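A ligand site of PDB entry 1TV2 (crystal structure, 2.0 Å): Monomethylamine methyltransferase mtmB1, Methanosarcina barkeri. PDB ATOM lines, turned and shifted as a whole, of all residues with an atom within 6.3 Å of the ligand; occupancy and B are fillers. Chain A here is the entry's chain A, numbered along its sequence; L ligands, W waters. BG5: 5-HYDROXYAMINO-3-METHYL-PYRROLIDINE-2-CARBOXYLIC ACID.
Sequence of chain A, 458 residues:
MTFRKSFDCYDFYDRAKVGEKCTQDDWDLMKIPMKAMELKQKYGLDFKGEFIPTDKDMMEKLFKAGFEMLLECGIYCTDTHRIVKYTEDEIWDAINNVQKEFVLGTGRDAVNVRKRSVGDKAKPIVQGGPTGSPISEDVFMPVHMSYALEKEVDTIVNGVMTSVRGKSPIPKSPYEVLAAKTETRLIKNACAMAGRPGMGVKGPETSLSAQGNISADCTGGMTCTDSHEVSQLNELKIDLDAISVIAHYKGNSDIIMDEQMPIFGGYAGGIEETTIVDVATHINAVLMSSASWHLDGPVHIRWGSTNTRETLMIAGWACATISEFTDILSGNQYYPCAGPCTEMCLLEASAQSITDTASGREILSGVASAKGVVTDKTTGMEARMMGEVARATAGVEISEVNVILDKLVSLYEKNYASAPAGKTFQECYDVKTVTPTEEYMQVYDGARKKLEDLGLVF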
ATOM      1  N   GLN A 127       3.252  15.404  21.524  1.00  0.00           N
ATOM      2  CA  GLN A 127       3.744  15.590  20.165  1.00  0.00           C
ATOM      3  C   GLN A 127       4.604  16.855  20.158  1.00  0.00           C
ATOM      4  O   GLN A 127       4.076  17.962  20.157  1.00  0.00           O
ATOM      5  CB  GLN A 127       2.569  15.742  19.204  1.00  0.00           C
ATOM      6  CG  GLN A 127       2.959  15.915  17.761  1.00  0.00           C
ATOM      7  CD  GLN A 127       1.816  15.581  16.823  1.00  0.00           C
ATOM      8  OE1 GLN A 127       0.956  16.424  16.527  1.00  0.00           O
ATOM      9  NE2 GLN A 127       1.778  14.338  16.371  1.00  0.00           N
ATOM     10  N   PRO A 130       8.968  21.890  16.216  1.00  0.00           N
ATOM     11  CA  PRO A 130       8.923  23.329  15.924  1.00  0.00           C
ATOM     12  C   PRO A 130       7.485  23.810  15.761  1.00  0.00           C
ATOM     13  O   PRO A 130       7.209  25.000  15.760  1.00  0.00           O
ATOM     14  CB  PRO A 130       9.736  23.443  14.626  1.00  0.00           C
ATOM     15  CG  PRO A 130      10.740  22.333  14.772  1.00  0.00           C
ATOM     16  CD  PRO A 130       9.878  21.199  15.278  1.00  0.00           C
ATOM     17  N   THR A 131       6.572  22.853  15.603  1.00  0.00           N
ATOM     18  CA  THR A 131       5.164  23.172  15.466  1.00  0.00           C
ATOM     19  C   THR A 131       4.914  24.158  14.322  1.00  0.00           C
ATOM     20  O   THR A 131       4.324  25.223  14.513  1.00  0.00           O
ATOM     21  CB  THR A 131       4.607  23.728  16.810  1.00  0.00           C
ATOM     22  OG1 THR A 131       5.030  22.869  17.878  1.00  0.00           O
ATOM     23  CG2 THR A 131       3.087  23.775  16.805  1.00  0.00           C
ATOM     24  N   GLY A 132       5.378  23.793  13.134  1.00  0.00           N
ATOM     25  CA  GLY A 132       5.179  24.620  11.946  1.00  0.00           C
ATOM     26  C   GLY A 132       5.961  25.911  11.877  1.00  0.00           C
ATOM     27  O   GLY A 132       5.753  26.694  10.948  1.00  0.00           O
ATOM     28  N   SER A 133       6.858  26.151  12.821  1.00  0.00           N
ATOM     29  CA  SER A 133       7.648  27.383  12.811  1.00  0.00           C
ATOM     30  C   SER A 133       8.785  27.298  11.804  1.00  0.00           C
ATOM     31  O   SER A 133       9.240  26.199  11.465  1.00  0.00           O
ATOM     32  CB  SER A 133       8.226  27.656  14.204  1.00  0.00           C
ATOM     33  OG  SER A 133       7.196  27.718  15.185  1.00  0.00           O
ATOM     34  N   VAL A 157       6.002  17.002  15.639  1.00  0.00           N
ATOM     35  CA  VAL A 157       5.173  17.902  14.838  1.00  0.00           C
ATOM     36  C   VAL A 157       6.199  18.709  14.062  1.00  0.00           C
ATOM     37  O   VAL A 157       6.992  19.463  14.642  1.00  0.00           O
ATOM     38  CB  VAL A 157       4.252  18.830  15.668  1.00  0.00           C
ATOM     39  CG1 VAL A 157       5.032  19.546  16.764  1.00  0.00           C
ATOM     40  CG2 VAL A 157       3.579  19.836  14.737  1.00  0.00           C
ATOM     41  N   ASN A 158       6.202  18.529  12.748  1.00  0.00           N
ATOM     42  CA  ASN A 158       7.162  19.164  11.848  1.00  0.00           C
ATOM     43  C   ASN A 158       7.278  20.683  11.842  1.00  0.00           C
ATOM     44  O   ASN A 158       6.307  21.408  12.058  1.00  0.00           O
ATOM     45  CB  ASN A 158       6.896  18.724  10.405  1.00  0.00           C
ATOM     46  CG  ASN A 158       6.992  17.210  10.221  1.00  0.00           C
ATOM     47  OD1 ASN A 158       7.225  16.466  11.172  1.00  0.00           O
ATOM     48  ND2 ASN A 158       6.796  16.754   8.987  1.00  0.00           N
ATOM     49  N   LYS A 202       3.859  14.613  12.211  1.00  0.00           N
ATOM     50  CA  LYS A 202       2.628  15.300  11.829  1.00  0.00           C
ATOM     51  C   LYS A 202       3.029  16.385  10.841  1.00  0.00           C
ATOM     52  O   LYS A 202       3.917  17.201  11.119  1.00  0.00           O
ATOM     53  CB  LYS A 202       1.930  15.914  13.045  1.00  0.00           C
ATOM     54  CG  LYS A 202       0.521  16.446  12.764  1.00  0.00           C
ATOM     55  CD  LYS A 202       0.482  17.956  12.490  1.00  0.00           C
ATOM     56  CE  LYS A 202       0.424  18.767  13.796  1.00  0.00           C
ATOM     57  NZ  LYS A 202       0.165  20.192  13.565  1.00  0.00           N
ATOM     58  N   GLY A 203       2.391  16.365   9.673  1.00  0.00           N
ATOM     59  CA  GLY A 203       2.672  17.339   8.639  1.00  0.00           C
ATOM     60  C   GLY A 203       1.748  17.038   7.463  1.00  0.00           C
ATOM     61  O   GLY A 203       0.692  16.442   7.678  1.00  0.00           O
ATOM     62  N   PRO A 204       2.098  17.438   6.226  1.00  0.00           N
ATOM     63  CA  PRO A 204       3.307  18.167   5.816  1.00  0.00           C
ATOM     64  C   PRO A 204       3.124  19.666   6.103  1.00  0.00           C
ATOM     65  O   PRO A 204       2.054  20.214   5.883  1.00  0.00           O
ATOM     66  CB  PRO A 204       3.375  17.867   4.322  1.00  0.00           C
ATOM     67  CG  PRO A 204       1.927  17.842   3.923  1.00  0.00           C
ATOM     68  CD  PRO A 204       1.282  17.054   5.056  1.00  0.00           C
ATOM     69  N   GLU A 205       4.175  20.315   6.594  1.00  0.00           N
ATOM     70  CA  GLU A 205       4.075  21.720   6.966  1.00  0.00           C
ATOM     71  C   GLU A 205       4.611  22.760   5.983  1.00  0.00           C
ATOM     72  O   GLU A 205       3.994  23.815   5.794  1.00  0.00           O
ATOM     73  CB  GLU A 205       4.727  21.942   8.328  1.00  0.00           C
ATOM     74  CG  GLU A 205       4.126  21.099   9.459  1.00  0.00           C
ATOM     75  CD  GLU A 205       2.617  21.230   9.543  1.00  0.00           C
ATOM     76  OE1 GLU A 205       2.093  22.330   9.265  1.00  0.00           O
ATOM     77  OE2 GLU A 205       1.953  20.226   9.894  1.00  0.00           O
ATOM     78  N   GLU A 229      -2.116  16.549   7.983  1.00  0.00           N
ATOM     79  CA  GLU A 229      -2.858  17.776   8.249  1.00  0.00           C
ATOM     80  C   GLU A 229      -3.678  18.383   7.127  1.00  0.00           C
ATOM     81  O   GLU A 229      -3.286  18.380   5.966  1.00  0.00           O
ATOM     82  CB  GLU A 229      -1.906  18.851   8.780  1.00  0.00           C
ATOM     83  CG  GLU A 229      -0.952  19.479   7.736  1.00  0.00           C
ATOM     84  CD  GLU A 229      -1.603  20.589   6.898  1.00  0.00           C
ATOM     85  OE1 GLU A 229      -2.429  21.339   7.456  1.00  0.00           O
ATOM     86  OE2 GLU A 229      -1.269  20.731   5.696  1.00  0.00           O
ATOM     87  N   VAL A 230      -4.831  18.897   7.519  1.00  0.00           N
ATOM     88  CA  VAL A 230      -5.736  19.608   6.626  1.00  0.00           C
ATOM     89  C   VAL A 230      -6.330  20.677   7.553  1.00  0.00           C
ATOM     90  O   VAL A 230      -6.724  20.375   8.681  1.00  0.00           O
ATOM     91  CB  VAL A 230      -6.846  18.696   6.027  1.00  0.00           C
ATOM     92  CG1 VAL A 230      -7.754  18.157   7.122  1.00  0.00           C
ATOM     93  CG2 VAL A 230      -7.649  19.489   4.996  1.00  0.00           C
ATOM     94  N   SER A 231      -6.362  21.922   7.082  1.00  0.00           N
ATOM     95  CA  SER A 231      -6.867  23.015   7.907  1.00  0.00           C
ATOM     96  C   SER A 231      -8.206  23.602   7.497  1.00  0.00           C
ATOM     97  O   SER A 231      -8.422  23.908   6.330  1.00  0.00           O
ATOM     98  CB  SER A 231      -5.852  24.155   7.939  1.00  0.00           C
ATOM     99  OG  SER A 231      -4.578  23.708   8.375  1.00  0.00           O
ATOM    100  N   MET A 257      -5.524  14.336  10.334  1.00  0.00           N
ATOM    101  CA  MET A 257      -5.661  15.284  11.422  1.00  0.00           C
ATOM    102  C   MET A 257      -6.268  16.566  10.859  1.00  0.00           C
ATOM    103  O   MET A 257      -5.605  17.284  10.110  1.00  0.00           O
ATOM    104  CB  MET A 257      -4.326  15.629  12.065  1.00  0.00           C
ATOM    105  CG  MET A 257      -4.481  16.651  13.191  1.00  0.00           C
ATOM    106  SD  MET A 257      -2.996  17.598  13.565  1.00  0.00           S
ATOM    107  CE  MET A 257      -3.024  18.769  12.214  1.00  0.00           C
ATOM    108  N   GLU A 259      -7.550  20.291  11.446  1.00  0.00           N
ATOM    109  CA  GLU A 259      -7.266  21.336  12.412  1.00  0.00           C
ATOM    110  C   GLU A 259      -8.126  22.577  12.183  1.00  0.00           C
ATOM    111  O   GLU A 259      -8.621  22.816  11.080  1.00  0.00           O
ATOM    112  CB  GLU A 259      -5.797  21.775  12.348  1.00  0.00           C
ATOM    113  CG  GLU A 259      -5.588  22.944  11.398  1.00  0.00           C
ATOM    114  CD  GLU A 259      -4.396  23.802  11.759  1.00  0.00           C
ATOM    115  OE1 GLU A 259      -4.220  24.127  12.951  1.00  0.00           O
ATOM    116  OE2 GLU A 259      -3.629  24.165  10.836  1.00  0.00           O
ATOM    117  N   MET A 261      -8.382  26.715  14.156  1.00  0.00           N
ATOM    118  CA  MET A 261      -8.008  27.626  15.229  1.00  0.00           C
ATOM    119  C   MET A 261      -9.052  28.718  15.378  1.00  0.00           C
ATOM    120  O   MET A 261      -8.936  29.786  14.760  1.00  0.00           O
ATOM    121  CB  MET A 261      -6.637  28.243  14.942  1.00  0.00           C
ATOM    122  CG  MET A 261      -5.477  27.259  14.943  1.00  0.00           C
ATOM    123  SD  MET A 261      -3.892  28.104  14.815  1.00  0.00           S
ATOM    124  CE  MET A 261      -3.558  28.474  16.542  1.00  0.00           C
ATOM    125  N   TRP A 293      -8.598  12.396  13.978  1.00  0.00           N
ATOM    126  CA  TRP A 293      -8.584  13.233  15.171  1.00  0.00           C
ATOM    127  C   TRP A 293      -8.576  14.710  14.778  1.00  0.00           C
ATOM    128  O   TRP A 293      -8.213  15.055  13.649  1.00  0.00           O
ATOM    129  CB  TRP A 293      -7.393  12.916  16.105  1.00  0.00           C
ATOM    130  CG  TRP A 293      -5.999  13.174  15.584  1.00  0.00           C
ATOM    131  CD1 TRP A 293      -5.297  12.398  14.708  1.00  0.00           C
ATOM    132  CD2 TRP A 293      -5.097  14.209  16.019  1.00  0.00           C
ATOM    133  NE1 TRP A 293      -4.008  12.883  14.577  1.00  0.00           N
ATOM    134  CE2 TRP A 293      -3.868  13.994  15.365  1.00  0.00           C
ATOM    135  CE3 TRP A 293      -5.223  15.304  16.896  1.00  0.00           C
ATOM    136  CZ2 TRP A 293      -2.754  14.830  15.565  1.00  0.00           C
ATOM    137  CZ3 TRP A 293      -4.111  16.131  17.096  1.00  0.00           C
ATOM    138  CH2 TRP A 293      -2.897  15.886  16.425  1.00  0.00           C
ATOM    139  N   LEU A 295      -7.376  18.705  15.697  1.00  0.00           N
ATOM    140  CA  LEU A 295      -6.450  19.583  16.401  1.00  0.00           C
ATOM    141  C   LEU A 295      -7.101  20.955  16.574  1.00  0.00           C
ATOM    142  O   LEU A 295      -7.411  21.625  15.587  1.00  0.00           O
ATOM    143  CB  LEU A 295      -5.140  19.733  15.620  1.00  0.00           C
ATOM    144  CG  LEU A 295      -4.068  20.574  16.311  1.00  0.00           C
ATOM    145  CD1 LEU A 295      -3.520  19.810  17.513  1.00  0.00           C
ATOM    146  CD2 LEU A 295      -2.949  20.885  15.325  1.00  0.00           C
ATOM    147  N   ASN A 332      -4.551  19.779  20.946  1.00  0.00           N
ATOM    148  CA  ASN A 332      -4.519  21.236  20.933  1.00  0.00           C
ATOM    149  C   ASN A 332      -3.080  21.663  20.629  1.00  0.00           C
ATOM    150  O   ASN A 332      -2.131  20.968  21.030  1.00  0.00           O
ATOM    151  CB  ASN A 332      -4.983  21.783  22.298  1.00  0.00           C
ATOM    152  CG  ASN A 332      -5.356  23.252  22.240  1.00  0.00           C
ATOM    153  OD1 ASN A 332      -5.477  23.845  21.164  1.00  0.00           O
ATOM    154  ND2 ASN A 332      -5.568  23.860  23.409  1.00  0.00           N
ATOM    155  N   GLN A 333      -2.916  22.772  19.918  1.00  0.00           N
ATOM    156  CA  GLN A 333      -1.595  23.278  19.545  1.00  0.00           C
ATOM    157  C   GLN A 333      -1.178  24.464  20.409  1.00  0.00           C
ATOM    158  O   GLN A 333      -2.000  25.276  20.833  1.00  0.00           O
ATOM    159  CB  GLN A 333      -1.566  23.639  18.062  1.00  0.00           C
ATOM    160  CG  GLN A 333      -2.605  24.655  17.636  1.00  0.00           C
ATOM    161  CD  GLN A 333      -2.809  24.667  16.126  1.00  0.00           C
ATOM    162  OE1 GLN A 333      -1.910  25.006  15.368  1.00  0.00           O
ATOM    163  NE2 GLN A 333      -4.008  24.290  15.699  1.00  0.00           N
ATOM    164  N   TYR A 334       0.136  24.564  20.635  1.00  0.00           N
ATOM    165  CA  TYR A 334       0.710  25.582  21.508  1.00  0.00           C
ATOM    166  C   TYR A 334       1.393  26.787  20.862  1.00  0.00           C
ATOM    167  O   TYR A 334       2.390  26.645  20.154  1.00  0.00           O
ATOM    168  CB  TYR A 334       1.712  24.893  22.457  1.00  0.00           C
ATOM    169  CG  TYR A 334       1.067  23.914  23.414  1.00  0.00           C
ATOM    170  CD1 TYR A 334       0.270  22.864  22.939  1.00  0.00           C
ATOM    171  CD2 TYR A 334       1.208  24.062  24.795  1.00  0.00           C
ATOM    172  CE1 TYR A 334      -0.371  21.991  23.826  1.00  0.00           C
ATOM    173  CE2 TYR A 334       0.576  23.188  25.688  1.00  0.00           C
ATOM    174  CZ  TYR A 334      -0.221  22.168  25.197  1.00  0.00           C
ATOM    175  OH  TYR A 334      -0.896  21.348  26.069  1.00  0.00           O
ATOM    176  N   TYR A 335       0.853  27.972  21.138  1.00  0.00           N
ATOM    177  CA  TYR A 335       1.404  29.221  20.619  1.00  0.00           C
ATOM    178  C   TYR A 335       1.603  30.253  21.723  1.00  0.00           C
ATOM    179  O   TYR A 335       0.727  31.091  21.970  1.00  0.00           O
ATOM    180  CB  TYR A 335       0.479  29.823  19.552  1.00  0.00           C
ATOM    181  CG  TYR A 335       0.651  29.227  18.181  1.00  0.00           C
ATOM    182  CD1 TYR A 335      -0.002  28.048  17.820  1.00  0.00           C
ATOM    183  CD2 TYR A 335       1.444  29.858  17.228  1.00  0.00           C
ATOM    184  CE1 TYR A 335       0.140  27.511  16.542  1.00  0.00           C
ATOM    185  CE2 TYR A 335       1.605  29.330  15.959  1.00  0.00           C
ATOM    186  CZ  TYR A 335       0.942  28.163  15.615  1.00  0.00           C
ATOM    187  OH  TYR A 335       1.092  27.656  14.349  1.00  0.00           O
ATOM    188  N   SER A 365       0.235  19.115  21.046  1.00  0.00           N
ATOM    189  CA  SER A 365       1.144  19.391  19.938  1.00  0.00           C
ATOM    190  C   SER A 365       1.801  20.779  20.086  1.00  0.00           C
ATOM    191  O   SER A 365       1.167  21.802  19.845  1.00  0.00           O
ATOM    192  CB  SER A 365       0.359  19.307  18.619  1.00  0.00           C
ATOM    193  OG  SER A 365       1.213  19.175  17.494  1.00  0.00           O
ATOM    194  N   GLY A 366       3.072  20.784  20.486  1.00  0.00           N
ATOM    195  CA  GLY A 366       3.793  22.036  20.667  1.00  0.00           C
ATOM    196  C   GLY A 366       5.304  21.855  20.613  1.00  0.00           C
ATOM    197  O   GLY A 366       5.777  20.735  20.453  1.00  0.00           O
ATOM    198  N   ALA A 368       5.048  26.070  19.502  1.00  0.00           N
ATOM    199  CA  ALA A 368       5.366  27.116  18.550  1.00  0.00           C
ATOM    200  C   ALA A 368       5.738  28.390  19.305  1.00  0.00           C
ATOM    201  O   ALA A 368       4.989  29.380  19.304  1.00  0.00           O
ATOM    202  CB  ALA A 368       4.171  27.374  17.635  1.00  0.00           C
HETATM  203  C1  BG5 L   1       0.319  21.158  14.486  1.00  0.00           C
HETATM  204  C2  BG5 L   1       0.063  22.590  14.021  1.00  0.00           C
HETATM  205  C3  BG5 L   1       1.340  23.269  13.588  1.00  0.00           C
HETATM  206  C4  BG5 L   1       1.356  23.205  12.056  1.00  0.00           C
HETATM  207  C5  BG5 L   1      -0.105  23.117  11.611  1.00  0.00           C
HETATM  208  C6  BG5 L   1       1.263  24.608  14.087  1.00  0.00           C
HETATM  209  N1  BG5 L   1      -0.897  22.674  12.834  1.00  0.00           N
HETATM  210  O1  BG5 L   1       0.565  20.941  15.671  1.00  0.00           O
HETATM  211  N2  BG5 L   1      -0.242  22.114  10.599  1.00  0.00           N
HETATM  212  O2  BG5 L   1      -0.471  20.700  10.805  1.00  0.00           O
HETATM  213  O   HOH W   1      -0.292  24.219   8.494  1.00  0.00           O
HETATM  214  O   HOH W   2      -1.824  25.974  12.538  1.00  0.00           O
HETATM  215  O   HOH W   3      -2.873  21.899  10.076  1.00  0.00           O
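Water W3 lies within hydrogen-bond range of the side-chain carboxylate of Glu 259, a nitrogen (N2) of the ligand, the side-chain carboxylate of Glu 229 and the side-chain hydroxyl of Ser 231.
Water W1 lies within hydrogen-bond range of N2 of the ligand and OE1 of Glu 205.
NE2 of Gln 333 sits at hydrogen-bond distance from OE1 of Glu 259 (2.8 Å).
OG of Ser 231 lies within hydrogen-bond range of OE1 of Glu 229 (3.3 Å).
The backbone NH (N) of Glu 229 sits at hydrogen-bond distance from the backbone carbonyl oxygen (O) of Gly 203 (2.8 Å).
OG of Ser 365 is in hydrogen-bond range of OE1 of Gln 127 (2.9 Å).
OG of Ser 231 is in hydrogen-bond range of OE2 of Glu 259.
The backbone NH (N) of Ser 365 is in hydrogen-bond range of the backbone carbonyl oxygen (O) of Asn 332 (3.0 Å).
The backbone NH of Val 230 is in hydrogen-bond range of the backbone carbonyl oxygen of Met 257 (3.1 Å).
OE1 of Gln 333 sits close to SD of Met 261 (3.7 Å).
A carbon (C1) of the ligand is bonded to the side-chain amino group of Lys 202, 1.3 Å away.
OG of Ser 365 lies within hydrogen-bond range of O1 of the ligand, at 2.6 Å.
The side-chain carboxylate (OE2) of Glu 205 is in hydrogen-bond range of an oxygen (O2) of the ligand (2.6 Å).
OE1 of Glu 259 lies within salt-bridge range of N1 of the ligand (3.6 Å).
Thr 131 touches the ligand.
Val 157 touches the ligand.
Glu 229 touches the ligand (CB to O2, 3.1 Å).
CE of Met 257 touches O2 of the ligand, at 3.5 Å.
Leu 295 touches the ligand (CD2 to C1, 3.4 Å).
Gln 333 touches the ligand (OE1 to C2, 3.4 Å).
Tyr 335 touches the ligand.
Hydrophobic or aromatic side chains that line the ligand: Val 157, Met 257, Leu 295 and Tyr 335.
11 residues have an atom within 4 Å of the ligand: Thr 131, Val 157, Lys 202, Glu 205, Glu 229, Met 257, Glu 259, Leu 295, Gln 333, Tyr 335 and Ser 365.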
